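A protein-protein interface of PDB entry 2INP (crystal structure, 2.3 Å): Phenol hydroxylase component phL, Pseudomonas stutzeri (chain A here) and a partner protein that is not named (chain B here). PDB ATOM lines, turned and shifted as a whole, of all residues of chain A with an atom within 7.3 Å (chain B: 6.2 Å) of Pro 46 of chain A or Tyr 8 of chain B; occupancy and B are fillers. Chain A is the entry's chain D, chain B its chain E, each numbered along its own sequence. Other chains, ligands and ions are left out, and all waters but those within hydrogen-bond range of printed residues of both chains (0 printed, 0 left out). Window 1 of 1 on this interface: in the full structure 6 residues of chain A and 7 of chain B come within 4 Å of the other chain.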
ATOM      1  N   PHE A  42      17.668  -0.169 -19.552  1.00  0.00           N
ATOM      2  CA  PHE A  42      18.120   0.631 -20.710  1.00  0.00           C
ATOM      3  C   PHE A  42      18.418  -0.335 -21.873  1.00  0.00           C
ATOM      4  O   PHE A  42      18.844  -1.495 -21.670  1.00  0.00           O
ATOM      5  CB  PHE A  42      19.323   1.535 -20.363  1.00  0.00           C
ATOM      6  CG  PHE A  42      18.988   2.538 -19.303  1.00  0.00           C
ATOM      7  CD1 PHE A  42      19.402   2.344 -17.966  1.00  0.00           C
ATOM      8  CD2 PHE A  42      18.111   3.630 -19.604  1.00  0.00           C
ATOM      9  CE1 PHE A  42      19.001   3.274 -16.977  1.00  0.00           C
ATOM     10  CE2 PHE A  42      17.679   4.487 -18.604  1.00  0.00           C
ATOM     11  CZ  PHE A  42      18.128   4.325 -17.306  1.00  0.00           C
ATOM     12  N   HIS A  43      18.156   0.131 -23.091  1.00  0.00           N
ATOM     13  CA  HIS A  43      18.109  -0.765 -24.215  1.00  0.00           C
ATOM     14  C   HIS A  43      19.469  -0.961 -24.919  1.00  0.00           C
ATOM     15  O   HIS A  43      19.698  -2.015 -25.436  1.00  0.00           O
ATOM     16  CB  HIS A  43      16.960  -0.382 -25.165  1.00  0.00           C
ATOM     17  CG  HIS A  43      15.628  -0.848 -24.673  1.00  0.00           C
ATOM     18  ND1 HIS A  43      14.814  -0.078 -23.856  1.00  0.00           N
ATOM     19  CD2 HIS A  43      14.999  -2.030 -24.810  1.00  0.00           C
ATOM     20  CE1 HIS A  43      13.725  -0.768 -23.544  1.00  0.00           C
ATOM     21  NE2 HIS A  43      13.813  -1.962 -24.107  1.00  0.00           N
ATOM     22  N   TYR A  44      20.371   0.010 -24.891  1.00  0.00           N
ATOM     23  CA  TYR A  44      21.663  -0.071 -25.587  1.00  0.00           C
ATOM     24  C   TYR A  44      22.690   0.677 -24.794  1.00  0.00           C
ATOM     25  O   TYR A  44      22.347   1.694 -24.168  1.00  0.00           O
ATOM     26  CB  TYR A  44      21.564   0.607 -26.983  1.00  0.00           C
ATOM     27  CG  TYR A  44      20.189   0.468 -27.625  1.00  0.00           C
ATOM     28  CD1 TYR A  44      19.252   1.544 -27.576  1.00  0.00           C
ATOM     29  CD2 TYR A  44      19.840  -0.706 -28.297  1.00  0.00           C
ATOM     30  CE1 TYR A  44      18.003   1.428 -28.144  1.00  0.00           C
ATOM     31  CE2 TYR A  44      18.554  -0.864 -28.908  1.00  0.00           C
ATOM     32  CZ  TYR A  44      17.657   0.218 -28.833  1.00  0.00           C
ATOM     33  OH  TYR A  44      16.403   0.084 -29.396  1.00  0.00           O
ATOM     34  N   ARG A  45      23.949   0.228 -24.861  1.00  0.00           N
ATOM     35  CA  ARG A  45      25.046   0.909 -24.180  1.00  0.00           C
ATOM     36  C   ARG A  45      25.417   2.179 -24.944  1.00  0.00           C
ATOM     37  O   ARG A  45      25.384   2.140 -26.171  1.00  0.00           O
ATOM     38  CB  ARG A  45      26.259  -0.004 -24.039  1.00  0.00           C
ATOM     39  CG  ARG A  45      26.000  -1.241 -23.218  1.00  0.00           C
ATOM     40  CD  ARG A  45      25.769  -0.866 -21.778  1.00  0.00           C
ATOM     41  NE  ARG A  45      27.021  -0.498 -21.190  1.00  0.00           N
ATOM     42  CZ  ARG A  45      27.879  -1.375 -20.698  1.00  0.00           C
ATOM     43  NH1 ARG A  45      29.013  -0.953 -20.212  1.00  0.00           N
ATOM     44  NH2 ARG A  45      27.632  -2.674 -20.752  1.00  0.00           N
ATOM     45  N   PRO A  46      25.783   3.276 -24.229  1.00  0.00           N
ATOM     46  CA  PRO A  46      26.381   4.454 -24.837  1.00  0.00           C
ATOM     47  C   PRO A  46      27.517   4.135 -25.825  1.00  0.00           C
ATOM     48  O   PRO A  46      28.442   3.394 -25.491  1.00  0.00           O
ATOM     49  CB  PRO A  46      26.945   5.242 -23.642  1.00  0.00           C
ATOM     50  CG  PRO A  46      26.011   4.926 -22.535  1.00  0.00           C
ATOM     51  CD  PRO A  46      25.595   3.458 -22.765  1.00  0.00           C
ATOM     52  N   GLN A  47      27.451   4.721 -27.031  1.00  0.00           N
ATOM     53  CA  GLN A  47      28.499   4.554 -28.031  1.00  0.00           C
ATOM     54  C   GLN A  47      29.649   5.477 -27.650  1.00  0.00           C
ATOM     55  O   GLN A  47      30.748   5.352 -28.178  1.00  0.00           O
ATOM     56  CB  GLN A  47      27.939   4.885 -29.419  1.00  0.00           C
ATOM     57  CG  GLN A  47      26.960   3.827 -29.889  1.00  0.00           C
ATOM     58  CD  GLN A  47      26.082   4.349 -30.988  1.00  0.00           C
ATOM     59  OE1 GLN A  47      26.567   4.933 -32.014  1.00  0.00           O
ATOM     60  NE2 GLN A  47      24.769   4.137 -30.818  1.00  0.00           N
ATOM     61  N   TRP A  48      29.386   6.414 -26.730  1.00  0.00           N
ATOM     62  CA  TRP A  48      30.356   7.434 -26.328  1.00  0.00           C
ATOM     63  C   TRP A  48      31.051   7.169 -24.948  1.00  0.00           C
ATOM     64  O   TRP A  48      31.805   8.023 -24.388  1.00  0.00           O
ATOM     65  CB  TRP A  48      29.680   8.828 -26.468  1.00  0.00           C
ATOM     66  CG  TRP A  48      28.262   8.836 -25.957  1.00  0.00           C
ATOM     67  CD1 TRP A  48      27.156   8.652 -26.672  1.00  0.00           C
ATOM     68  CD2 TRP A  48      27.848   8.936 -24.580  1.00  0.00           C
ATOM     69  NE1 TRP A  48      26.055   8.672 -25.886  1.00  0.00           N
ATOM     70  CE2 TRP A  48      26.440   8.834 -24.576  1.00  0.00           C
ATOM     71  CE3 TRP A  48      28.544   9.092 -23.341  1.00  0.00           C
ATOM     72  CZ2 TRP A  48      25.664   8.858 -23.370  1.00  0.00           C
ATOM     73  CZ3 TRP A  48      27.805   9.107 -22.138  1.00  0.00           C
ATOM     74  CH2 TRP A  48      26.360   9.015 -22.163  1.00  0.00           C
ATOM     75  N   ASP A  49      30.865   5.969 -24.397  1.00  0.00           N
ATOM     76  CA  ASP A  49      31.345   5.701 -23.030  1.00  0.00           C
ATOM     77  C   ASP A  49      31.314   4.218 -22.882  1.00  0.00           C
ATOM     78  O   ASP A  49      30.239   3.655 -22.977  1.00  0.00           O
ATOM     79  CB  ASP A  49      30.397   6.339 -21.944  1.00  0.00           C
ATOM     80  CG  ASP A  49      30.871   6.117 -20.516  1.00  0.00           C
ATOM     81  OD1 ASP A  49      31.812   5.297 -20.310  1.00  0.00           O
ATOM     82  OD2 ASP A  49      30.313   6.784 -19.560  1.00  0.00           O
ATOM     83  N   SER A  50      32.476   3.587 -22.642  1.00  0.00           N
ATOM     84  CA  SER A  50      32.530   2.130 -22.457  1.00  0.00           C
ATOM     85  C   SER A  50      32.260   1.684 -21.034  1.00  0.00           C
ATOM     86  O   SER A  50      32.108   0.448 -20.813  1.00  0.00           O
ATOM     87  CB  SER A  50      33.884   1.548 -22.848  1.00  0.00           C
ATOM     88  OG  SER A  50      34.928   2.356 -22.354  1.00  0.00           O
ATOM     89  N   GLU A  51      32.206   2.644 -20.080  1.00  0.00           N
ATOM     90  CA  GLU A  51      32.322   2.296 -18.646  1.00  0.00           C
ATOM     91  C   GLU A  51      31.003   2.300 -17.929  1.00  0.00           C
ATOM     92  O   GLU A  51      30.903   1.720 -16.807  1.00  0.00           O
ATOM     93  CB  GLU A  51      33.365   3.154 -17.898  1.00  0.00           C
ATOM     94  CG  GLU A  51      34.818   3.016 -18.516  1.00  0.00           C
ATOM     95  CD  GLU A  51      35.360   1.518 -18.460  1.00  0.00           C
ATOM     96  OE1 GLU A  51      35.503   0.973 -17.324  1.00  0.00           O
ATOM     97  OE2 GLU A  51      35.635   0.886 -19.529  1.00  0.00           O
ATOM     98  N   HIS A  52      30.013   2.995 -18.509  1.00  0.00           N
ATOM     99  CA  HIS A  52      28.722   3.180 -17.813  1.00  0.00           C
ATOM    100  C   HIS A  52      27.582   3.065 -18.802  1.00  0.00           C
ATOM    101  O   HIS A  52      27.763   3.273 -20.014  1.00  0.00           O
ATOM    102  CB  HIS A  52      28.640   4.571 -17.100  1.00  0.00           C
ATOM    103  CG  HIS A  52      29.918   5.071 -16.506  1.00  0.00           C
ATOM    104  ND1 HIS A  52      30.329   4.746 -15.227  1.00  0.00           N
ATOM    105  CD2 HIS A  52      30.860   5.910 -16.996  1.00  0.00           C
ATOM    106  CE1 HIS A  52      31.468   5.368 -14.952  1.00  0.00           C
ATOM    107  NE2 HIS A  52      31.807   6.087 -16.007  1.00  0.00           N
ATOM    108  N   THR A  53      26.430   2.678 -18.265  1.00  0.00           N
ATOM    109  CA  THR A  53      25.144   2.713 -18.941  1.00  0.00           C
ATOM    110  C   THR A  53      24.582   4.171 -19.127  1.00  0.00           C
ATOM    111  O   THR A  53      25.151   5.163 -18.679  1.00  0.00           O
ATOM    112  CB  THR A  53      24.109   1.736 -18.225  1.00  0.00           C
ATOM    113  OG1 THR A  53      23.551   2.346 -17.052  1.00  0.00           O
ATOM    114  CG2 THR A  53      24.776   0.403 -17.806  1.00  0.00           C
ATOM    115  N   LEU A  54      23.492   4.295 -19.862  1.00  0.00           N
ATOM    116  CA  LEU A  54      22.633   5.487 -19.736  1.00  0.00           C
ATOM    117  C   LEU A  54      22.253   5.626 -18.245  1.00  0.00           C
ATOM    118  O   LEU A  54      22.130   4.624 -17.571  1.00  0.00           O
ATOM    119  CB  LEU A  54      21.379   5.312 -20.577  1.00  0.00           C
ATOM    120  CG  LEU A  54      21.244   5.840 -22.022  1.00  0.00           C
ATOM    121  CD1 LEU A  54      22.538   6.308 -22.707  1.00  0.00           C
ATOM    122  CD2 LEU A  54      20.281   5.046 -22.897  1.00  0.00           C
ATOM    123  N   ASN A  55      22.180   6.858 -17.714  1.00  0.00           N
ATOM    124  CA  ASN A  55      21.607   7.131 -16.362  1.00  0.00           C
ATOM    125  C   ASN A  55      22.205   6.208 -15.332  1.00  0.00           C
ATOM    126  O   ASN A  55      21.512   5.340 -14.782  1.00  0.00           O
ATOM    127  CB  ASN A  55      20.049   6.970 -16.391  1.00  0.00           C
ATOM    128  CG  ASN A  55      19.360   8.049 -17.234  1.00  0.00           C
ATOM    129  OD1 ASN A  55      20.046   8.906 -17.786  1.00  0.00           O
ATOM    130  ND2 ASN A  55      18.018   8.039 -17.318  1.00  0.00           N
ATOM    131  N   ARG A  59      28.828   7.049 -12.738  1.00  0.00           N
ATOM    132  CA  ARG A  59      29.566   8.169 -13.404  1.00  0.00           C
ATOM    133  C   ARG A  59      30.271   9.053 -12.363  1.00  0.00           C
ATOM    134  O   ARG A  59      31.179   9.789 -12.717  1.00  0.00           O
ATOM    135  CB  ARG A  59      28.638   9.031 -14.299  1.00  0.00           C
ATOM    136  CG  ARG A  59      28.251   8.426 -15.578  1.00  0.00           C
ATOM    137  CD  ARG A  59      27.872   9.416 -16.702  1.00  0.00           C
ATOM    138  NE  ARG A  59      27.988   8.669 -17.937  1.00  0.00           N
ATOM    139  CZ  ARG A  59      27.095   7.786 -18.359  1.00  0.00           C
ATOM    140  NH1 ARG A  59      27.337   7.086 -19.466  1.00  0.00           N
ATOM    141  NH2 ARG A  59      25.939   7.649 -17.715  1.00  0.00           N
ATOM    142  N   VAL B   2      28.330   0.092 -36.161  1.00  0.00           N
ATOM    143  CA  VAL B   2      28.199   1.156 -35.167  1.00  0.00           C
ATOM    144  C   VAL B   2      29.427   2.046 -35.176  1.00  0.00           C
ATOM    145  O   VAL B   2      30.561   1.541 -35.161  1.00  0.00           O
ATOM    146  CB  VAL B   2      27.975   0.540 -33.714  1.00  0.00           C
ATOM    147  CG1 VAL B   2      27.741   1.602 -32.705  1.00  0.00           C
ATOM    148  CG2 VAL B   2      26.739  -0.339 -33.697  1.00  0.00           C
ATOM    149  N   ASN B   3      29.241   3.355 -35.216  1.00  0.00           N
ATOM    150  CA  ASN B   3      30.296   4.243 -34.774  1.00  0.00           C
ATOM    151  C   ASN B   3      30.214   4.386 -33.240  1.00  0.00           C
ATOM    152  O   ASN B   3      29.076   4.527 -32.639  1.00  0.00           O
ATOM    153  CB  ASN B   3      30.197   5.593 -35.461  1.00  0.00           C
ATOM    154  CG  ASN B   3      30.268   5.470 -36.997  1.00  0.00           C
ATOM    155  OD1 ASN B   3      30.797   4.499 -37.518  1.00  0.00           O
ATOM    156  ND2 ASN B   3      29.691   6.443 -37.711  1.00  0.00           N
ATOM    157  N   ALA B   4      31.382   4.270 -32.609  1.00  0.00           N
ATOM    158  CA  ALA B   4      31.518   4.307 -31.178  1.00  0.00           C
ATOM    159  C   ALA B   4      32.909   4.783 -30.990  1.00  0.00           C
ATOM    160  O   ALA B   4      33.699   4.770 -31.936  1.00  0.00           O
ATOM    161  CB  ALA B   4      31.372   2.908 -30.576  1.00  0.00           C
ATOM    162  N   TYR B   6      34.908   3.287 -28.830  1.00  0.00           N
ATOM    163  CA  TYR B   6      35.634   2.133 -28.326  1.00  0.00           C
ATOM    164  C   TYR B   6      35.094   0.972 -29.137  1.00  0.00           C
ATOM    165  O   TYR B   6      34.210   1.158 -30.028  1.00  0.00           O
ATOM    166  CB  TYR B   6      35.387   1.938 -26.846  1.00  0.00           C
ATOM    167  CG  TYR B   6      33.907   1.782 -26.473  1.00  0.00           C
ATOM    168  CD1 TYR B   6      33.062   2.875 -26.364  1.00  0.00           C
ATOM    169  CD2 TYR B   6      33.361   0.517 -26.275  1.00  0.00           C
ATOM    170  CE1 TYR B   6      31.669   2.705 -26.006  1.00  0.00           C
ATOM    171  CE2 TYR B   6      32.002   0.327 -25.947  1.00  0.00           C
ATOM    172  CZ  TYR B   6      31.154   1.429 -25.772  1.00  0.00           C
ATOM    173  OH  TYR B   6      29.833   1.170 -25.408  1.00  0.00           O
ATOM    174  N   ASP B   7      35.612  -0.226 -28.871  1.00  0.00           N
ATOM    175  CA  ASP B   7      35.201  -1.358 -29.670  1.00  0.00           C
ATOM    176  C   ASP B   7      33.843  -1.833 -29.191  1.00  0.00           C
ATOM    177  O   ASP B   7      33.696  -2.385 -28.100  1.00  0.00           O
ATOM    178  CB  ASP B   7      36.254  -2.475 -29.687  1.00  0.00           C
ATOM    179  CG  ASP B   7      35.979  -3.463 -30.808  1.00  0.00           C
ATOM    180  OD1 ASP B   7      35.956  -3.041 -32.005  1.00  0.00           O
ATOM    181  OD2 ASP B   7      35.683  -4.636 -30.509  1.00  0.00           O
ATOM    182  N   TYR B   8      32.828  -1.571 -29.987  1.00  0.00           N
ATOM    183  CA  TYR B   8      31.454  -1.680 -29.510  1.00  0.00           C
ATOM    184  C   TYR B   8      30.967  -3.075 -29.758  1.00  0.00           C
ATOM    185  O   TYR B   8      30.517  -3.388 -30.857  1.00  0.00           O
ATOM    186  CB  TYR B   8      30.584  -0.667 -30.294  1.00  0.00           C
ATOM    187  CG  TYR B   8      29.240  -0.358 -29.700  1.00  0.00           C
ATOM    188  CD1 TYR B   8      29.096   0.586 -28.638  1.00  0.00           C
ATOM    189  CD2 TYR B   8      28.095  -0.946 -30.218  1.00  0.00           C
ATOM    190  CE1 TYR B   8      27.866   0.864 -28.092  1.00  0.00           C
ATOM    191  CE2 TYR B   8      26.847  -0.677 -29.670  1.00  0.00           C
ATOM    192  CZ  TYR B   8      26.746   0.253 -28.609  1.00  0.00           C
ATOM    193  OH  TYR B   8      25.501   0.520 -28.084  1.00  0.00           O
ATOM    194  N   LYS B   9      31.040  -3.934 -28.752  1.00  0.00           N
ATOM    195  CA  LYS B   9      30.713  -5.352 -28.982  1.00  0.00           C
ATOM    196  C   LYS B   9      30.148  -5.921 -27.705  1.00  0.00           C
ATOM    197  O   LYS B   9      30.776  -5.857 -26.659  1.00  0.00           O
ATOM    198  CB  LYS B   9      31.958  -6.138 -29.439  1.00  0.00           C
ATOM    199  CG  LYS B   9      31.982  -6.474 -30.992  1.00  0.00           C
ATOM    200  CD  LYS B   9      33.393  -6.942 -31.469  1.00  0.00           C
ATOM    201  CE  LYS B   9      33.848  -6.218 -32.770  1.00  0.00           C
ATOM    202  NZ  LYS B   9      33.126  -6.723 -33.973  1.00  0.00           N
ATOM    203  N   PHE B  10      28.925  -6.418 -27.774  1.00  0.00           N
ATOM    204  CA  PHE B  10      28.245  -6.841 -26.569  1.00  0.00           C
ATOM    205  C   PHE B  10      27.601  -8.171 -26.881  1.00  0.00           C
ATOM    206  O   PHE B  10      27.372  -8.495 -28.043  1.00  0.00           O
ATOM    207  CB  PHE B  10      27.181  -5.780 -26.116  1.00  0.00           C
ATOM    208  CG  PHE B  10      27.784  -4.428 -25.781  1.00  0.00           C
ATOM    209  CD1 PHE B  10      28.225  -4.150 -24.503  1.00  0.00           C
ATOM    210  CD2 PHE B  10      27.976  -3.478 -26.773  1.00  0.00           C
ATOM    211  CE1 PHE B  10      28.835  -2.931 -24.205  1.00  0.00           C
ATOM    212  CE2 PHE B  10      28.576  -2.280 -26.483  1.00  0.00           C
ATOM    213  CZ  PHE B  10      29.007  -2.000 -25.213  1.00  0.00           C
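Tyr 8 of chain B touches three residues of chain A.
Printed residues of chain B within 4 Å of Gln 47 of chain A: Val 2 (3.6 Å), Asn 3 (2.6 Å), Ala 4 (3.3 Å), Tyr 6 (3.5 Å) and Tyr 8 (3.6 Å).
Printed residues of chain B within 4 Å of Ser 50 of chain A: Tyr 6.
The nearest residue of chain B that does not touch Pro 46 of chain A is Phe 10 of chain B (5.4 Å).
The nearest printed residue of chain A that does not touch Tyr 6 of chain B is Arg 45 of chain A (4.003 Å).
Arg 45 of chain A touches Phe 10 of chain B.
Tyr 8 of chain B touches Pro 46 of chain A (CE1 to O, 3.7 Å).
Gln 47 of chain A touches Val 2 of chain B (OE1 to CG1, 3.6 Å).
Gln 47 of chain A touches Ala 4 of chain B (O to CA, 3.3 Å).
O of Gln 47 of chain A touches CE1 of Tyr 6 of chain B, at 3.5 Å.
Gln 47 of chain A touches Tyr 8 of chain B (CG to CE1, 3.6 Å).
Ser 50 of chain A touches Tyr 6 of chain B (N to CE1, 3.6 Å).
The guanidinium group of Arg 45 of chain A lies within hydrogen-bond range of the backbone carbonyl oxygen of Ser 50 of chain A (3.5 Å).
The side-chain carboxylate (OD1) of Asp 49 of chain A is in hydrogen-bond range of the backbone NH (N) of Glu 51 of chain A (2.7 Å).
OD1 of Asp 49 of chain A sits at hydrogen-bond distance from N of His 52 of chain A (3.4 Å).
The side-chain carboxylate (OD2) of Asp 49 of chain A lies within salt-bridge range of the guanidinium group (NH1) of Arg 59 of chain A (3.0 Å).
The side-chain hydroxyl (OG) of Ser 50 of chain A sits at hydrogen-bond distance from the side-chain carboxylate (OE2) of Glu 51 of chain A, at 3.3 Å.
The backbone carbonyl oxygen (O) of Arg 45 of chain A sits at hydrogen-bond distance from the side-chain hydroxyl (OH) of Tyr 8 of chain B.
The backbone carbonyl oxygen (O) of Pro 46 of chain A is in hydrogen-bond range of the side-chain hydroxyl (OH) of Tyr 6 of chain B, 2.6 Å away.
O of Asn 3 of chain B sits close to OE1 of Gln 47 of chain A (2.6 Å).
OH of Tyr 6 of chain B lies close to O of Asp 49 of chain A, at 3.5 Å.
Printed residues of chain B that touch a printed residue of chain A: Val 2, Asn 3, Ala 4, Tyr 6, Tyr 8 and Phe 10.
Hydrophobic or aromatic side chains of chain B that line the printed part of chain A: Val 2, Ala 4, Tyr 6, Tyr 8 and Phe 10.
Along chain B the printed residues that touch a printed residue of chain A span positions 2 to 10.
Printed residues of chain A that touch a printed residue of chain B: Arg 45, Pro 46, Gln 47, Asp 49 and Ser 50.
Among the printed residues, 11 pairs touch across the chains.
Among the printed residues, no Asp or Glu carboxylate lies within 4 Å of a Lys or Arg side-chain nitrogen of the other chain.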
